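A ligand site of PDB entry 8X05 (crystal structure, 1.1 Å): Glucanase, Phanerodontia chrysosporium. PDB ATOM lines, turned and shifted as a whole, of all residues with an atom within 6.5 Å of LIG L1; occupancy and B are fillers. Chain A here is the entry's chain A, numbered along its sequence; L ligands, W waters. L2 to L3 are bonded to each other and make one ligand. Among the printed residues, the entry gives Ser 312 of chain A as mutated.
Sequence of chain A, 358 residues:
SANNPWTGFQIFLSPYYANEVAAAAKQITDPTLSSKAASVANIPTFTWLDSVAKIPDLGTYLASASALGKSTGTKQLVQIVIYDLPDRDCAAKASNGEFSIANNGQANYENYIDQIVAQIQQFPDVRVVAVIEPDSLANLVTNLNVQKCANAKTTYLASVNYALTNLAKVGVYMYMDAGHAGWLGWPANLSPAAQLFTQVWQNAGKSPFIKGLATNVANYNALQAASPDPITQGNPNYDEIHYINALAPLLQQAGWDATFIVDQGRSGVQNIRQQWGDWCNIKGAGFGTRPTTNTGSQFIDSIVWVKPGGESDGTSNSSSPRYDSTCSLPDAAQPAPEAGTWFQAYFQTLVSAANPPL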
ATOM      1  N   TRP A  48     -25.498   6.368  -1.423  1.00  0.00           N
ATOM      2  CA  TRP A  48     -25.342   5.608  -0.198  1.00  0.00           C
ATOM      3  C   TRP A  48     -24.514   6.391   0.808  1.00  0.00           C
ATOM      4  O   TRP A  48     -23.400   6.825   0.503  1.00  0.00           O
ATOM      5  CB  TRP A  48     -24.683   4.266  -0.491  1.00  0.00           C
ATOM      6  CG  TRP A  48     -25.575   3.327  -1.256  1.00  0.00           C
ATOM      7  CD1 TRP A  48     -26.180   3.547  -2.473  1.00  0.00           C
ATOM      8  CD2 TRP A  48     -25.964   2.015  -0.854  1.00  0.00           C
ATOM      9  NE1 TRP A  48     -26.912   2.451  -2.850  1.00  0.00           N
ATOM     10  CE2 TRP A  48     -26.787   1.489  -1.876  1.00  0.00           C
ATOM     11  CE3 TRP A  48     -25.687   1.224   0.262  1.00  0.00           C
ATOM     12  CZ2 TRP A  48     -27.326   0.212  -1.800  1.00  0.00           C
ATOM     13  CZ3 TRP A  48     -26.225  -0.040   0.330  1.00  0.00           C
ATOM     14  CH2 TRP A  48     -27.038  -0.533  -0.693  1.00  0.00           C
ATOM     15  N   LEU A  49     -25.057   6.572   2.013  1.00  0.00           N
ATOM     16  CA  LEU A  49     -24.289   7.148   3.116  1.00  0.00           C
ATOM     17  C   LEU A  49     -23.638   5.986   3.874  1.00  0.00           C
ATOM     18  O   LEU A  49     -24.030   5.597   4.980  1.00  0.00           O
ATOM     19  CB  LEU A  49     -25.165   8.041   3.985  1.00  0.00           C
ATOM     20  CG  LEU A  49     -25.929   9.109   3.198  1.00  0.00           C
ATOM     21  CD1 LEU A  49     -26.781   9.967   4.117  1.00  0.00           C
ATOM     22  CD2 LEU A  49     -25.053   9.985   2.317  1.00  0.00           C
ATOM     23  N   ASP A  50     -22.648   5.365   3.211  1.00  0.00           N
ATOM     24  CA  ASP A  50     -22.014   4.146   3.692  1.00  0.00           C
ATOM     25  C   ASP A  50     -20.905   4.415   4.686  1.00  0.00           C
ATOM     26  O   ASP A  50     -20.289   3.468   5.183  1.00  0.00           O
ATOM     27  CB  ASP A  50     -21.547   3.295   2.503  1.00  0.00           C
ATOM     28  CG  ASP A  50     -20.474   3.963   1.683  1.00  0.00           C
ATOM     29  OD1 ASP A  50     -20.597   5.170   1.397  1.00  0.00           O
ATOM     30  OD2 ASP A  50     -19.505   3.276   1.281  1.00  0.00           O
ATOM     31  N   LYS A  54     -19.469  10.467   4.220  1.00  0.00           N
ATOM     32  CA  LYS A  54     -20.431  10.847   3.195  1.00  0.00           C
ATOM     33  C   LYS A  54     -21.435  11.888   3.703  1.00  0.00           C
ATOM     34  O   LYS A  54     -22.185  12.450   2.899  1.00  0.00           O
ATOM     35  CB  LYS A  54     -21.187   9.624   2.662  1.00  0.00           C
ATOM     36  CG  LYS A  54     -20.317   8.507   2.099  1.00  0.00           C
ATOM     37  CD  LYS A  54     -19.520   8.943   0.874  1.00  0.00           C
ATOM     38  CE  LYS A  54     -18.704   7.780   0.294  1.00  0.00           C
ATOM     39  NZ  LYS A  54     -19.537   6.851  -0.528  1.00  0.00           N
ATOM     40  N   TYR A  83     -26.741   3.375   5.631  1.00  0.00           N
ATOM     41  CA  TYR A  83     -26.029   2.098   5.519  1.00  0.00           C
ATOM     42  C   TYR A  83     -24.717   2.162   6.309  1.00  0.00           C
ATOM     43  O   TYR A  83     -23.619   2.171   5.747  1.00  0.00           O
ATOM     44  CB  TYR A  83     -25.785   1.723   4.061  1.00  0.00           C
ATOM     45  CG  TYR A  83     -25.219   0.330   3.874  1.00  0.00           C
ATOM     46  CD1 TYR A  83     -25.919  -0.789   4.337  1.00  0.00           C
ATOM     47  CD2 TYR A  83     -23.995   0.128   3.242  1.00  0.00           C
ATOM     48  CE1 TYR A  83     -25.414  -2.073   4.167  1.00  0.00           C
ATOM     49  CE2 TYR A  83     -23.490  -1.144   3.065  1.00  0.00           C
ATOM     50  CZ  TYR A  83     -24.191  -2.238   3.524  1.00  0.00           C
ATOM     51  OH  TYR A  83     -23.673  -3.503   3.334  1.00  0.00           O
ATOM     52  N   ARG A  88     -21.951  -4.205  10.499  1.00  0.00           N
ATOM     53  CA  ARG A  88     -22.726  -4.213   9.256  1.00  0.00           C
ATOM     54  C   ARG A  88     -22.482  -5.513   8.485  1.00  0.00           C
ATOM     55  O   ARG A  88     -21.388  -6.090   8.528  1.00  0.00           O
ATOM     56  CB  ARG A  88     -22.307  -3.023   8.389  1.00  0.00           C
ATOM     57  CG  ARG A  88     -23.274  -2.620   7.311  1.00  0.00           C
ATOM     58  CD  ARG A  88     -22.825  -1.336   6.604  1.00  0.00           C
ATOM     59  NE  ARG A  88     -21.574  -1.514   5.859  1.00  0.00           N
ATOM     60  CZ  ARG A  88     -20.866  -0.528   5.346  1.00  0.00           C
ATOM     61  NH1 ARG A  88     -21.265   0.733   5.439  1.00  0.00           N
ATOM     62  NH2 ARG A  88     -19.719  -0.802   4.716  1.00  0.00           N
ATOM     63  N   ALA A  94     -18.199  -9.149   2.829  1.00  0.00           N
ATOM     64  CA  ALA A  94     -17.774  -8.224   1.772  1.00  0.00           C
ATOM     65  C   ALA A  94     -17.983  -6.760   2.138  1.00  0.00           C
ATOM     66  O   ALA A  94     -17.212  -5.904   1.689  1.00  0.00           O
ATOM     67  CB  ALA A  94     -18.525  -8.543   0.482  1.00  0.00           C
ATOM     68  N   SER A  95     -19.012  -6.454   2.918  1.00  0.00           N
ATOM     69  CA  SER A  95     -19.403  -5.068   3.151  1.00  0.00           C
ATOM     70  C   SER A  95     -19.324  -4.670   4.625  1.00  0.00           C
ATOM     71  O   SER A  95     -20.035  -3.764   5.057  1.00  0.00           O
ATOM     72  CB  SER A  95     -20.763  -4.747   2.549  1.00  0.00           C
ATOM     73  OG  SER A  95     -20.635  -4.625   1.136  1.00  0.00           O
ATOM     74  N   ASN A  96     -18.475  -5.341   5.402  1.00  0.00           N
ATOM     75  CA  ASN A  96     -18.202  -4.881   6.754  1.00  0.00           C
ATOM     76  C   ASN A  96     -17.839  -3.398   6.727  1.00  0.00           C
ATOM     77  O   ASN A  96     -17.162  -2.917   5.804  1.00  0.00           O
ATOM     78  CB  ASN A  96     -17.089  -5.713   7.368  1.00  0.00           C
ATOM     79  CG  ASN A  96     -17.492  -7.162   7.588  1.00  0.00           C
ATOM     80  OD1 ASN A  96     -18.668  -7.525   7.461  1.00  0.00           O
ATOM     81  ND2 ASN A  96     -16.518  -7.997   7.896  1.00  0.00           N
ATOM     82  N   ALA A 218     -29.580  -4.110  -4.348  1.00  0.00           N
ATOM     83  CA  ALA A 218     -28.317  -4.749  -4.691  1.00  0.00           C
ATOM     84  C   ALA A 218     -28.488  -6.178  -5.201  1.00  0.00           C
ATOM     85  O   ALA A 218     -27.521  -6.949  -5.244  1.00  0.00           O
ATOM     86  CB  ALA A 218     -27.265  -4.681  -3.580  1.00  0.00           C
ATOM     87  N   VAL A 306     -31.453   1.458  -6.666  1.00  0.00           N
ATOM     88  CA  VAL A 306     -30.896   1.722  -5.342  1.00  0.00           C
ATOM     89  C   VAL A 306     -29.400   1.432  -5.361  1.00  0.00           C
ATOM     90  O   VAL A 306     -28.592   2.329  -5.114  1.00  0.00           O
ATOM     91  CB  VAL A 306     -31.610   0.942  -4.232  1.00  0.00           C
ATOM     92  CG1 VAL A 306     -31.078   1.360  -2.875  1.00  0.00           C
ATOM     93  CG2 VAL A 306     -33.124   1.172  -4.310  1.00  0.00           C
ATOM     94  N   LYS A 307     -29.014   0.180  -5.615  1.00  0.00           N
ATOM     95  CA  LYS A 307     -27.600  -0.141  -5.793  1.00  0.00           C
ATOM     96  C   LYS A 307     -27.112   0.518  -7.075  1.00  0.00           C
ATOM     97  O   LYS A 307     -27.707   0.302  -8.137  1.00  0.00           O
ATOM     98  CB  LYS A 307     -27.416  -1.655  -5.865  1.00  0.00           C
ATOM     99  CG  LYS A 307     -26.034  -2.130  -6.299  1.00  0.00           C
ATOM    100  CD  LYS A 307     -24.986  -1.906  -5.225  1.00  0.00           C
ATOM    101  CE  LYS A 307     -23.619  -2.320  -5.745  1.00  0.00           C
ATOM    102  NZ  LYS A 307     -22.548  -2.315  -4.698  1.00  0.00           N
ATOM    103  N   PRO A 308     -26.051   1.329  -7.021  1.00  0.00           N
ATOM    104  CA  PRO A 308     -25.597   2.026  -8.239  1.00  0.00           C
ATOM    105  C   PRO A 308     -24.731   1.085  -9.056  1.00  0.00           C
ATOM    106  O   PRO A 308     -23.634   0.701  -8.642  1.00  0.00           O
ATOM    107  CB  PRO A 308     -24.772   3.205  -7.678  1.00  0.00           C
ATOM    108  CG  PRO A 308     -25.111   3.265  -6.204  1.00  0.00           C
ATOM    109  CD  PRO A 308     -25.329   1.821  -5.845  1.00  0.00           C
ATOM    110  N   GLU A 311     -20.632  -0.021  -9.039  1.00  0.00           N
ATOM    111  CA  GLU A 311     -19.988  -0.092  -7.744  1.00  0.00           C
ATOM    112  C   GLU A 311     -19.979  -1.545  -7.286  1.00  0.00           C
ATOM    113  O   GLU A 311     -21.010  -2.206  -7.286  1.00  0.00           O
ATOM    114  CB  GLU A 311     -20.797   0.814  -6.816  1.00  0.00           C
ATOM    115  CG  GLU A 311     -20.428   2.269  -7.004  1.00  0.00           C
ATOM    116  CD  GLU A 311     -21.241   3.221  -6.146  1.00  0.00           C
ATOM    117  OE1 GLU A 311     -21.462   4.359  -6.583  1.00  0.00           O
ATOM    118  OE2 GLU A 311     -21.816   2.762  -5.124  1.00  0.00           O
ATOM    119  N   SER A 312     -18.790  -2.062  -6.934  1.00  0.00           N
ATOM    120  CA  SER A 312     -18.615  -3.484  -6.642  1.00  0.00           C
ATOM    121  C   SER A 312     -19.435  -3.913  -5.421  1.00  0.00           C
ATOM    122  O   SER A 312     -19.693  -3.120  -4.498  1.00  0.00           O
ATOM    123  CB  SER A 312     -17.138  -3.809  -6.381  1.00  0.00           C
ATOM    124  OG  SER A 312     -16.960  -5.180  -6.044  1.00  0.00           O
ATOM    125  N   ASP A 313     -19.831  -5.182  -5.411  1.00  0.00           N
ATOM    126  CA  ASP A 313     -20.461  -5.810  -4.253  1.00  0.00           C
ATOM    127  C   ASP A 313     -19.449  -6.419  -3.293  1.00  0.00           C
ATOM    128  O   ASP A 313     -19.844  -6.838  -2.192  1.00  0.00           O
ATOM    129  CB  ASP A 313     -21.378  -6.951  -4.716  1.00  0.00           C
ATOM    130  CG  ASP A 313     -22.492  -6.482  -5.598  1.00  0.00           C
ATOM    131  OD1 ASP A 313     -23.135  -5.461  -5.245  1.00  0.00           O
ATOM    132  OD2 ASP A 313     -22.732  -7.113  -6.650  1.00  0.00           O
ATOM    133  N   GLY A 314     -18.186  -6.519  -3.693  1.00  0.00           N
ATOM    134  CA  GLY A 314     -17.220  -7.186  -2.842  1.00  0.00           C
ATOM    135  C   GLY A 314     -15.983  -7.620  -3.595  1.00  0.00           C
ATOM    136  O   GLY A 314     -16.042  -7.885  -4.805  1.00  0.00           O
ATOM    137  N   ARG A 322     -12.125  -8.462   3.922  1.00  0.00           N
ATOM    138  CA  ARG A 322     -13.515  -8.472   3.510  1.00  0.00           C
ATOM    139  C   ARG A 322     -13.804  -9.495   2.416  1.00  0.00           C
ATOM    140  O   ARG A 322     -14.811  -9.382   1.710  1.00  0.00           O
ATOM    141  CB  ARG A 322     -14.023  -7.069   3.138  1.00  0.00           C
ATOM    142  CG  ARG A 322     -13.766  -6.042   4.249  1.00  0.00           C
ATOM    143  CD  ARG A 322     -14.704  -4.847   4.121  1.00  0.00           C
ATOM    144  NE  ARG A 322     -14.534  -4.151   2.848  1.00  0.00           N
ATOM    145  CZ  ARG A 322     -15.385  -3.241   2.371  1.00  0.00           C
ATOM    146  NH1 ARG A 322     -16.438  -2.852   3.082  1.00  0.00           N
ATOM    147  NH2 ARG A 322     -15.183  -2.740   1.156  1.00  0.00           N
ATOM    148  N   ALA A 339     -15.871  -3.832  -2.105  1.00  0.00           N
ATOM    149  CA  ALA A 339     -17.272  -3.405  -2.156  1.00  0.00           C
ATOM    150  C   ALA A 339     -17.383  -1.894  -2.059  1.00  0.00           C
ATOM    151  O   ALA A 339     -16.699  -1.252  -1.261  1.00  0.00           O
ATOM    152  CB  ALA A 339     -18.061  -4.059  -1.018  1.00  0.00           C
ATOM    153  N   GLY A 340     -18.238  -1.332  -2.907  1.00  0.00           N
ATOM    154  CA  GLY A 340     -18.446   0.094  -2.923  1.00  0.00           C
ATOM    155  C   GLY A 340     -17.512   0.866  -3.837  1.00  0.00           C
ATOM    156  O   GLY A 340     -17.777   2.045  -4.097  1.00  0.00           O
ATOM    157  N   THR A 341     -16.438   0.259  -4.317  1.00  0.00           N
ATOM    158  CA  THR A 341     -15.533   0.962  -5.207  1.00  0.00           C
ATOM    159  C   THR A 341     -15.877   0.657  -6.662  1.00  0.00           C
ATOM    160  O   THR A 341     -16.586  -0.303  -6.969  1.00  0.00           O
ATOM    161  CB  THR A 341     -14.061   0.617  -4.902  1.00  0.00           C
ATOM    162  OG1 THR A 341     -13.793  -0.738  -5.270  1.00  0.00           O
ATOM    163  CG2 THR A 341     -13.789   0.782  -3.415  1.00  0.00           C
HETATM  164  C1  LIG L   1     -20.903  -1.272  -0.350  1.00  0.00           C
HETATM  165  C2  LIG L   1     -21.094   0.177  -0.065  1.00  0.00           C
HETATM  166  C3  LIG L   1     -21.745   0.916  -1.201  1.00  0.00           C
HETATM  167  C4  LIG L   1     -22.989   0.192  -1.706  1.00  0.00           C
HETATM  168  C5  LIG L   1     -23.466   0.837  -2.966  1.00  0.00           C
HETATM  169  C6  LIG L   1     -22.183  -1.916  -0.831  1.00  0.00           C
HETATM  170  O1  LIG L   1     -22.007  -3.213  -1.197  1.00  0.00           O
HETATM  171  O2  LIG L   1     -20.463  -1.932   0.849  1.00  0.00           O
HETATM  172  O3  LIG L   1     -19.810   0.787   0.233  1.00  0.00           O
HETATM  173  O4  LIG L   1     -22.119   2.227  -0.765  1.00  0.00           O
HETATM  174  O5  LIG L   1     -22.672  -1.194  -2.043  1.00  0.00           O
HETATM  175  O6  LIG L   1     -22.614   0.503  -4.026  1.00  0.00           O
HETATM  176  C1  LG2 L   2     -30.227 -15.962   0.190  1.00  0.00           C
HETATM  177  C2  LG2 L   2     -30.341 -14.674  -0.618  1.00  0.00           C
HETATM  178  C3  LG2 L   2     -29.141 -13.829  -0.483  1.00  0.00           C
HETATM  179  C4  LG2 L   2     -28.817 -13.542   0.957  1.00  0.00           C
HETATM  180  C5  LG2 L   2     -28.811 -14.813   1.820  1.00  0.00           C
HETATM  181  C6  LG2 L   2     -28.729 -14.393   3.264  1.00  0.00           C
HETATM  182  O1  LG2 L   2     -29.178 -16.675  -0.270  1.00  0.00           O
HETATM  183  O2  LG2 L   2     -30.508 -14.982  -2.005  1.00  0.00           O
HETATM  184  O3  LG2 L   2     -29.420 -12.603  -1.216  1.00  0.00           O
HETATM  185  O4  LG2 L   2     -27.490 -13.038   1.071  1.00  0.00           O
HETATM  186  O5  LG2 L   2     -29.998 -15.658   1.636  1.00  0.00           O
HETATM  187  O6  LG2 L   2     -27.946 -15.287   4.016  1.00  0.00           O
HETATM  188  C1  LG3 L   3     -26.024 -11.224   1.672  1.00  0.00           C
HETATM  189  C2  LG3 L   3     -25.800  -9.755   1.604  1.00  0.00           C
HETATM  190  C3  LG3 L   3     -26.170  -9.172   0.265  1.00  0.00           C
HETATM  191  C4  LG3 L   3     -27.607  -9.559  -0.119  1.00  0.00           C
HETATM  192  C5  LG3 L   3     -27.971  -9.082  -1.498  1.00  0.00           C
HETATM  193  C6  LG3 L   3     -27.398 -11.624   1.176  1.00  0.00           C
HETATM  194  O1  LG3 L   3     -25.862 -11.696   3.036  1.00  0.00           O
HETATM  195  O2  LG3 L   3     -24.409  -9.473   1.898  1.00  0.00           O
HETATM  196  O3  LG3 L   3     -26.006  -7.748   0.265  1.00  0.00           O
HETATM  197  O4  LG3 L   3     -27.685 -11.021  -0.132  1.00  0.00           O
HETATM  198  O5  LG3 L   3     -29.278  -9.488  -1.840  1.00  0.00           O
HETATM  199  O   HOH W   1     -23.543  -4.346  -2.982  1.00  0.00           O
HETATM  200  O   HOH W   2     -18.059  -1.095   1.701  1.00  0.00           O
HETATM  201  O   HOH W   3     -18.452   1.387   3.117  1.00  0.00           O
HETATM  202  O   HOH W   4     -23.759  -4.483   0.658  1.00  0.00           O
HETATM  203  O   HOH W   5     -21.681   4.074  -2.772  1.00  0.00           O
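The side-chain carboxylate of Glu 311 is in hydrogen-bond range of an oxygen (O6) of LIG L1 (2.6 Å). An oxygen (O5) of LIG L1 lies within hydrogen-bond range of the side-chain amino group (NZ) of Lys 307, at 2.9 Å. The side-chain hydroxyl of Ser 95 sits at hydrogen-bond distance from an oxygen (O2) of LIG L1, at 2.7 Å. The side-chain carboxylate of Asp 50 is in hydrogen-bond range of an oxygen (O3) of LIG L1 (2.7 Å).
O of Glu 311 lies within hydrogen-bond range of NZ of Lys 307 (3.0 Å). O of Asp 50 sits at hydrogen-bond distance from NH1 of Arg 88, at 2.9 Å. The backbone carbonyl oxygen (O) of Ser 95 lies within hydrogen-bond range of the guanidinium group (NE) of Arg 88 (2.8 Å). The indole nitrogen (NE1) of Trp 48 sits at hydrogen-bond distance from the backbone carbonyl oxygen (O) of Val 306 (2.8 Å). N of Gly 340 sits at hydrogen-bond distance from O of Ser 312. The backbone carbonyl oxygen (O) of Tyr 83 is in hydrogen-bond range of the guanidinium group (NH1) of Arg 88, 2.8 Å away. The side-chain amino group (NZ) of Lys 54 is in salt-bridge range of the side-chain carboxylate (OD1) of Asp 50. The guanidinium group (NH2) of Arg 322 sits at hydrogen-bond distance from the backbone carbonyl oxygen (O) of Ala 339 (3.2 Å).
Residues that only touch LIG L1: Trp 48 (3.3 Å), Tyr 83 (3.8 Å), Pro 308 (3.5 Å), Ala 339 (3.7 Å) and Gly 340 (3.5 Å). Hydrophobic or aromatic side chains within 4 Å of LIG L1: Trp 48, Tyr 83, Pro 308 and Ala 339. Of the 21 residues printed, 9 come within 4 Å of LIG L1.
Water W1 lies within hydrogen-bond range of OD1 of Asp 313 (2.6 Å), O1 of LIG L1 (2.6 Å) and NZ of Lys 307 (2.8 Å). Water W2 lies within hydrogen-bond range of O2 of LIG L1 (2.7 Å), NH1 of Arg 322 (2.8 Å), O of Ala 339 (3.3 Å) and NH2 of Arg 88 (3.5 Å). Water W5 bridges the side-chain carboxylate (OE2) of Glu 311 and an oxygen (O4) of LIG L1. Water W4 lies within hydrogen-bond range of an oxygen (O1) of LIG L1, the side-chain hydroxyl (OH) of Tyr 83 and the side-chain hydroxyl (OG) of Ser 95. Water W3 lies within hydrogen-bond range of OD2 of Asp 50, NH2 of Arg 88 and O3 of LIG L1.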
